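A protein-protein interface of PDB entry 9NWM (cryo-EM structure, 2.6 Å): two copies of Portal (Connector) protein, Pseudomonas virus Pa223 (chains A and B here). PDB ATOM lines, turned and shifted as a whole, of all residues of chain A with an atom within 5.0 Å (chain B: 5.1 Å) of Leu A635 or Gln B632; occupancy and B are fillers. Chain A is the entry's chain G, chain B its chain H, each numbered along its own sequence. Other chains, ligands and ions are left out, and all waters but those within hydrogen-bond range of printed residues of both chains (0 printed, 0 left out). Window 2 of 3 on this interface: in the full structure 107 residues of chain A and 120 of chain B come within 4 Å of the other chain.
Among the printed residues, merely in contact across the chains: Arg A634 with Val B629 (3.2 Å), Glu A637 with Ile B633 (3.2 Å), Ile A638 with Gln B632 (3.2 Å) and Ile A638 with Ala B636 (3.5 Å).
Of chain A, only Arg A634, Leu A635 and Ile A638 come within 4 Å of Gln B632. Printed residues of chain B within 4 Å of Glu A637: Ile B633. Of the printed residues of chain A, Ile B633 touches Arg A634 and Glu A637. Of the printed residues of chain A, Ala B636 touches Ile A638 (3.5 Å). Ala A631 touches none of the printed residues of chain B. The nearest printed residue of chain B that does not touch Leu A635 is Ile B633 (5.7 Å).
Arg A634 touches Ile B633, but with the chains exchanged Ile A633 does not touch Arg B634 (10.2 Å). Positions printed for both chains: 631, 633, 634, 635 and 636. Of the 8 pairs that touch across the chains among the printed residues, none has its exchanged pair printed and touching as well.
Printed residues of chain A that touch a printed residue of chain B: Arg A634, Leu A635, Glu A637 and Ile A638. Of the 9 printed residues of chain B, 5 touch a printed residue of chain A. Hydrophobic or aromatic side chains of chain B that line the printed part of chain A: Val B629, Ile B633 and Ala B636. Among the printed residues, 8 pairs touch across the chains.
The backbone carbonyl oxygen (O) of Gln B628 sits at hydrogen-bond distance from the guanidinium group (NH1) of Arg A634. NH1 of Arg A634 is in hydrogen-bond range of OE1 of Gln B632, 2.5 Å away. The backbone NH of Leu A635 lies close to the side-chain amide nitrogen of Gln B632 (3.4 Å). The guanidinium group (NH1) of Arg A634 sits close to the backbone NH (N) of Ile B633.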
ATOM      1  N   ALA A 631       5.107  12.548 -30.201  1.00  0.00           N
ATOM      2  CA  ALA A 631       5.882  12.583 -28.966  1.00  0.00           C
ATOM      3  C   ALA A 631       6.420  13.980 -28.674  1.00  0.00           C
ATOM      4  O   ALA A 631       6.266  14.488 -27.556  1.00  0.00           O
ATOM      5  CB  ALA A 631       7.027  11.573 -29.037  1.00  0.00           C
ATOM      6  N   ILE A 633       6.247  17.031 -30.946  1.00  0.00           N
ATOM      7  CA  ILE A 633       5.804  18.198 -31.699  1.00  0.00           C
ATOM      8  C   ILE A 633       4.575  18.840 -31.079  1.00  0.00           C
ATOM      9  O   ILE A 633       4.168  19.922 -31.508  1.00  0.00           O
ATOM     10  CB  ILE A 633       5.536  17.862 -33.183  1.00  0.00           C
ATOM     11  CG1 ILE A 633       5.780  19.092 -34.060  1.00  0.00           C
ATOM     12  CG2 ILE A 633       4.103  17.405 -33.386  1.00  0.00           C
ATOM     13  CD1 ILE A 633       7.210  19.569 -34.066  1.00  0.00           C
ATOM     14  N   ARG A 634       3.990  18.217 -30.061  1.00  0.00           N
ATOM     15  CA  ARG A 634       2.748  18.667 -29.452  1.00  0.00           C
ATOM     16  C   ARG A 634       2.947  19.172 -28.032  1.00  0.00           C
ATOM     17  O   ARG A 634       2.454  20.252 -27.688  1.00  0.00           O
ATOM     18  CB  ARG A 634       1.734  17.517 -29.475  1.00  0.00           C
ATOM     19  CG  ARG A 634       1.591  16.867 -30.844  1.00  0.00           C
ATOM     20  CD  ARG A 634       0.218  16.254 -31.045  1.00  0.00           C
ATOM     21  NE  ARG A 634       0.182  14.847 -30.667  1.00  0.00           N
ATOM     22  CZ  ARG A 634      -0.798  14.287 -29.971  1.00  0.00           C
ATOM     23  NH1 ARG A 634      -1.835  14.992 -29.549  1.00  0.00           N
ATOM     24  NH2 ARG A 634      -0.735  12.989 -29.690  1.00  0.00           N
ATOM     25  N   LEU A 635       3.665  18.420 -27.195  1.00  0.00           N
ATOM     26  CA  LEU A 635       3.918  18.863 -25.827  1.00  0.00           C
ATOM     27  C   LEU A 635       4.794  20.109 -25.800  1.00  0.00           C
ATOM     28  O   LEU A 635       4.646  20.963 -24.915  1.00  0.00           O
ATOM     29  CB  LEU A 635       4.570  17.735 -25.026  1.00  0.00           C
ATOM     30  CG  LEU A 635       3.682  16.547 -24.657  1.00  0.00           C
ATOM     31  CD1 LEU A 635       4.523  15.399 -24.123  1.00  0.00           C
ATOM     32  CD2 LEU A 635       2.635  16.962 -23.637  1.00  0.00           C
ATOM     33  N   ALA A 636       5.719  20.225 -26.757  1.00  0.00           N
ATOM     34  CA  ALA A 636       6.647  21.352 -26.765  1.00  0.00           C
ATOM     35  C   ALA A 636       5.913  22.676 -26.926  1.00  0.00           C
ATOM     36  O   ALA A 636       6.233  23.657 -26.246  1.00  0.00           O
ATOM     37  CB  ALA A 636       7.680  21.172 -27.876  1.00  0.00           C
ATOM     38  N   GLU A 637       4.933  22.732 -27.827  1.00  0.00           N
ATOM     39  CA  GLU A 637       4.137  23.943 -27.973  1.00  0.00           C
ATOM     40  C   GLU A 637       3.079  24.086 -26.887  1.00  0.00           C
ATOM     41  O   GLU A 637       2.604  25.202 -26.650  1.00  0.00           O
ATOM     42  CB  GLU A 637       3.476  23.979 -29.354  1.00  0.00           C
ATOM     43  CG  GLU A 637       2.576  22.795 -29.654  1.00  0.00           C
ATOM     44  CD  GLU A 637       1.132  23.055 -29.276  1.00  0.00           C
ATOM     45  OE1 GLU A 637       0.696  24.222 -29.355  1.00  0.00           O
ATOM     46  OE2 GLU A 637       0.434  22.093 -28.897  1.00  0.00           O
ATOM     47  N   ILE A 638       2.695  22.990 -26.228  1.00  0.00           N
ATOM     48  CA  ILE A 638       1.737  23.077 -25.130  1.00  0.00           C
ATOM     49  C   ILE A 638       2.374  23.746 -23.919  1.00  0.00           C
ATOM     50  O   ILE A 638       1.772  24.619 -23.282  1.00  0.00           O
ATOM     51  CB  ILE A 638       1.189  21.682 -24.781  1.00  0.00           C
ATOM     52  CG1 ILE A 638       0.163  21.239 -25.822  1.00  0.00           C
ATOM     53  CG2 ILE A 638       0.570  21.676 -23.391  1.00  0.00           C
ATOM     54  CD1 ILE A 638      -0.375  19.849 -25.594  1.00  0.00           C
ATOM     55  N   GLU A 639       3.606  23.352 -23.585  1.00  0.00           N
ATOM     56  CA  GLU A 639       4.256  23.911 -22.404  1.00  0.00           C
ATOM     57  C   GLU A 639       4.561  25.395 -22.573  1.00  0.00           C
ATOM     58  O   GLU A 639       4.711  26.112 -21.577  1.00  0.00           O
ATOM     59  CB  GLU A 639       5.533  23.134 -22.079  1.00  0.00           C
ATOM     60  CG  GLU A 639       6.587  23.160 -23.172  1.00  0.00           C
ATOM     61  CD  GLU A 639       7.624  24.244 -22.958  1.00  0.00           C
ATOM     62  OE1 GLU A 639       7.612  24.878 -21.883  1.00  0.00           O
ATOM     63  OE2 GLU A 639       8.455  24.461 -23.866  1.00  0.00           O
ATOM     64  N   GLN B 628      -5.088   9.907 -29.652  1.00  0.00           N
ATOM     65  CA  GLN B 628      -4.262  10.730 -28.778  1.00  0.00           C
ATOM     66  C   GLN B 628      -4.208  12.172 -29.267  1.00  0.00           C
ATOM     67  O   GLN B 628      -4.057  13.097 -28.462  1.00  0.00           O
ATOM     68  CB  GLN B 628      -2.852  10.147 -28.681  1.00  0.00           C
ATOM     69  CG  GLN B 628      -2.776   8.834 -27.923  1.00  0.00           C
ATOM     70  CD  GLN B 628      -1.576   8.001 -28.324  1.00  0.00           C
ATOM     71  OE1 GLN B 628      -1.053   8.137 -29.430  1.00  0.00           O
ATOM     72  NE2 GLN B 628      -1.131   7.131 -27.425  1.00  0.00           N
ATOM     73  N   VAL B 629      -4.319  12.376 -30.582  1.00  0.00           N
ATOM     74  CA  VAL B 629      -4.367  13.734 -31.121  1.00  0.00           C
ATOM     75  C   VAL B 629      -5.579  14.480 -30.575  1.00  0.00           C
ATOM     76  O   VAL B 629      -5.456  15.597 -30.060  1.00  0.00           O
ATOM     77  CB  VAL B 629      -4.362  13.712 -32.660  1.00  0.00           C
ATOM     78  CG1 VAL B 629      -4.790  15.061 -33.212  1.00  0.00           C
ATOM     79  CG2 VAL B 629      -2.982  13.353 -33.174  1.00  0.00           C
ATOM     80  N   GLU B 630      -6.768  13.874 -30.661  1.00  0.00           N
ATOM     81  CA  GLU B 630      -7.917  14.509 -30.011  1.00  0.00           C
ATOM     82  C   GLU B 630      -7.709  14.633 -28.506  1.00  0.00           C
ATOM     83  O   GLU B 630      -8.202  15.580 -27.881  1.00  0.00           O
ATOM     84  CB  GLU B 630      -9.245  13.790 -30.280  1.00  0.00           C
ATOM     85  CG  GLU B 630      -9.896  14.052 -31.635  1.00  0.00           C
ATOM     86  CD  GLU B 630      -9.632  12.988 -32.661  1.00  0.00           C
ATOM     87  OE1 GLU B 630      -9.049  11.951 -32.303  1.00  0.00           O
ATOM     88  OE2 GLU B 630     -10.033  13.188 -33.827  1.00  0.00           O
ATOM     89  N   ALA B 631      -6.985  13.691 -27.904  1.00  0.00           N
ATOM     90  CA  ALA B 631      -6.849  13.694 -26.452  1.00  0.00           C
ATOM     91  C   ALA B 631      -5.873  14.758 -25.958  1.00  0.00           C
ATOM     92  O   ALA B 631      -6.004  15.229 -24.823  1.00  0.00           O
ATOM     93  CB  ALA B 631      -6.412  12.313 -25.964  1.00  0.00           C
ATOM     94  N   GLN B 632      -4.894  15.152 -26.779  1.00  0.00           N
ATOM     95  CA  GLN B 632      -3.766  15.929 -26.282  1.00  0.00           C
ATOM     96  C   GLN B 632      -3.539  17.270 -26.973  1.00  0.00           C
ATOM     97  O   GLN B 632      -3.293  18.259 -26.275  1.00  0.00           O
ATOM     98  CB  GLN B 632      -2.478  15.093 -26.377  1.00  0.00           C
ATOM     99  CG  GLN B 632      -1.240  15.722 -25.764  1.00  0.00           C
ATOM    100  CD  GLN B 632      -0.407  16.464 -26.785  1.00  0.00           C
ATOM    101  OE1 GLN B 632      -0.804  16.602 -27.940  1.00  0.00           O
ATOM    102  NE2 GLN B 632       0.766  16.926 -26.370  1.00  0.00           N
ATOM    103  N   ILE B 633      -3.616  17.344 -28.307  1.00  0.00           N
ATOM    104  CA  ILE B 633      -3.298  18.585 -29.015  1.00  0.00           C
ATOM    105  C   ILE B 633      -4.407  19.623 -28.901  1.00  0.00           C
ATOM    106  O   ILE B 633      -4.248  20.748 -29.395  1.00  0.00           O
ATOM    107  CB  ILE B 633      -2.995  18.311 -30.505  1.00  0.00           C
ATOM    108  CG1 ILE B 633      -2.189  19.455 -31.130  1.00  0.00           C
ATOM    109  CG2 ILE B 633      -4.282  18.149 -31.290  1.00  0.00           C
ATOM    110  CD1 ILE B 633      -0.835  19.669 -30.520  1.00  0.00           C
ATOM    111  N   ARG B 634      -5.511  19.299 -28.234  1.00  0.00           N
ATOM    112  CA  ARG B 634      -6.698  20.139 -28.270  1.00  0.00           C
ATOM    113  C   ARG B 634      -6.940  20.873 -26.957  1.00  0.00           C
ATOM    114  O   ARG B 634      -6.937  22.105 -26.942  1.00  0.00           O
ATOM    115  CB  ARG B 634      -7.907  19.272 -28.638  1.00  0.00           C
ATOM    116  CG  ARG B 634      -7.844  18.725 -30.052  1.00  0.00           C
ATOM    117  CD  ARG B 634      -9.043  17.853 -30.352  1.00  0.00           C
ATOM    118  NE  ARG B 634     -10.293  18.599 -30.375  1.00  0.00           N
ATOM    119  CZ  ARG B 634     -11.489  18.035 -30.453  1.00  0.00           C
ATOM    120  NH1 ARG B 634     -11.631  16.720 -30.506  1.00  0.00           N
ATOM    121  NH2 ARG B 634     -12.571  18.806 -30.467  1.00  0.00           N
ATOM    122  N   LEU B 635      -7.090  20.150 -25.842  1.00  0.00           N
ATOM    123  CA  LEU B 635      -7.517  20.781 -24.593  1.00  0.00           C
ATOM    124  C   LEU B 635      -6.567  21.894 -24.164  1.00  0.00           C
ATOM    125  O   LEU B 635      -6.968  22.828 -23.456  1.00  0.00           O
ATOM    126  CB  LEU B 635      -7.634  19.726 -23.492  1.00  0.00           C
ATOM    127  CG  LEU B 635      -8.749  18.690 -23.655  1.00  0.00           C
ATOM    128  CD1 LEU B 635      -8.763  17.723 -22.480  1.00  0.00           C
ATOM    129  CD2 LEU B 635     -10.103  19.366 -23.817  1.00  0.00           C
ATOM    130  N   ALA B 636      -5.305  21.815 -24.592  1.00  0.00           N
ATOM    131  CA  ALA B 636      -4.329  22.833 -24.224  1.00  0.00           C
ATOM    132  C   ALA B 636      -4.701  24.200 -24.786  1.00  0.00           C
ATOM    133  O   ALA B 636      -4.548  25.219 -24.105  1.00  0.00           O
ATOM    134  CB  ALA B 636      -2.938  22.421 -24.700  1.00  0.00           C
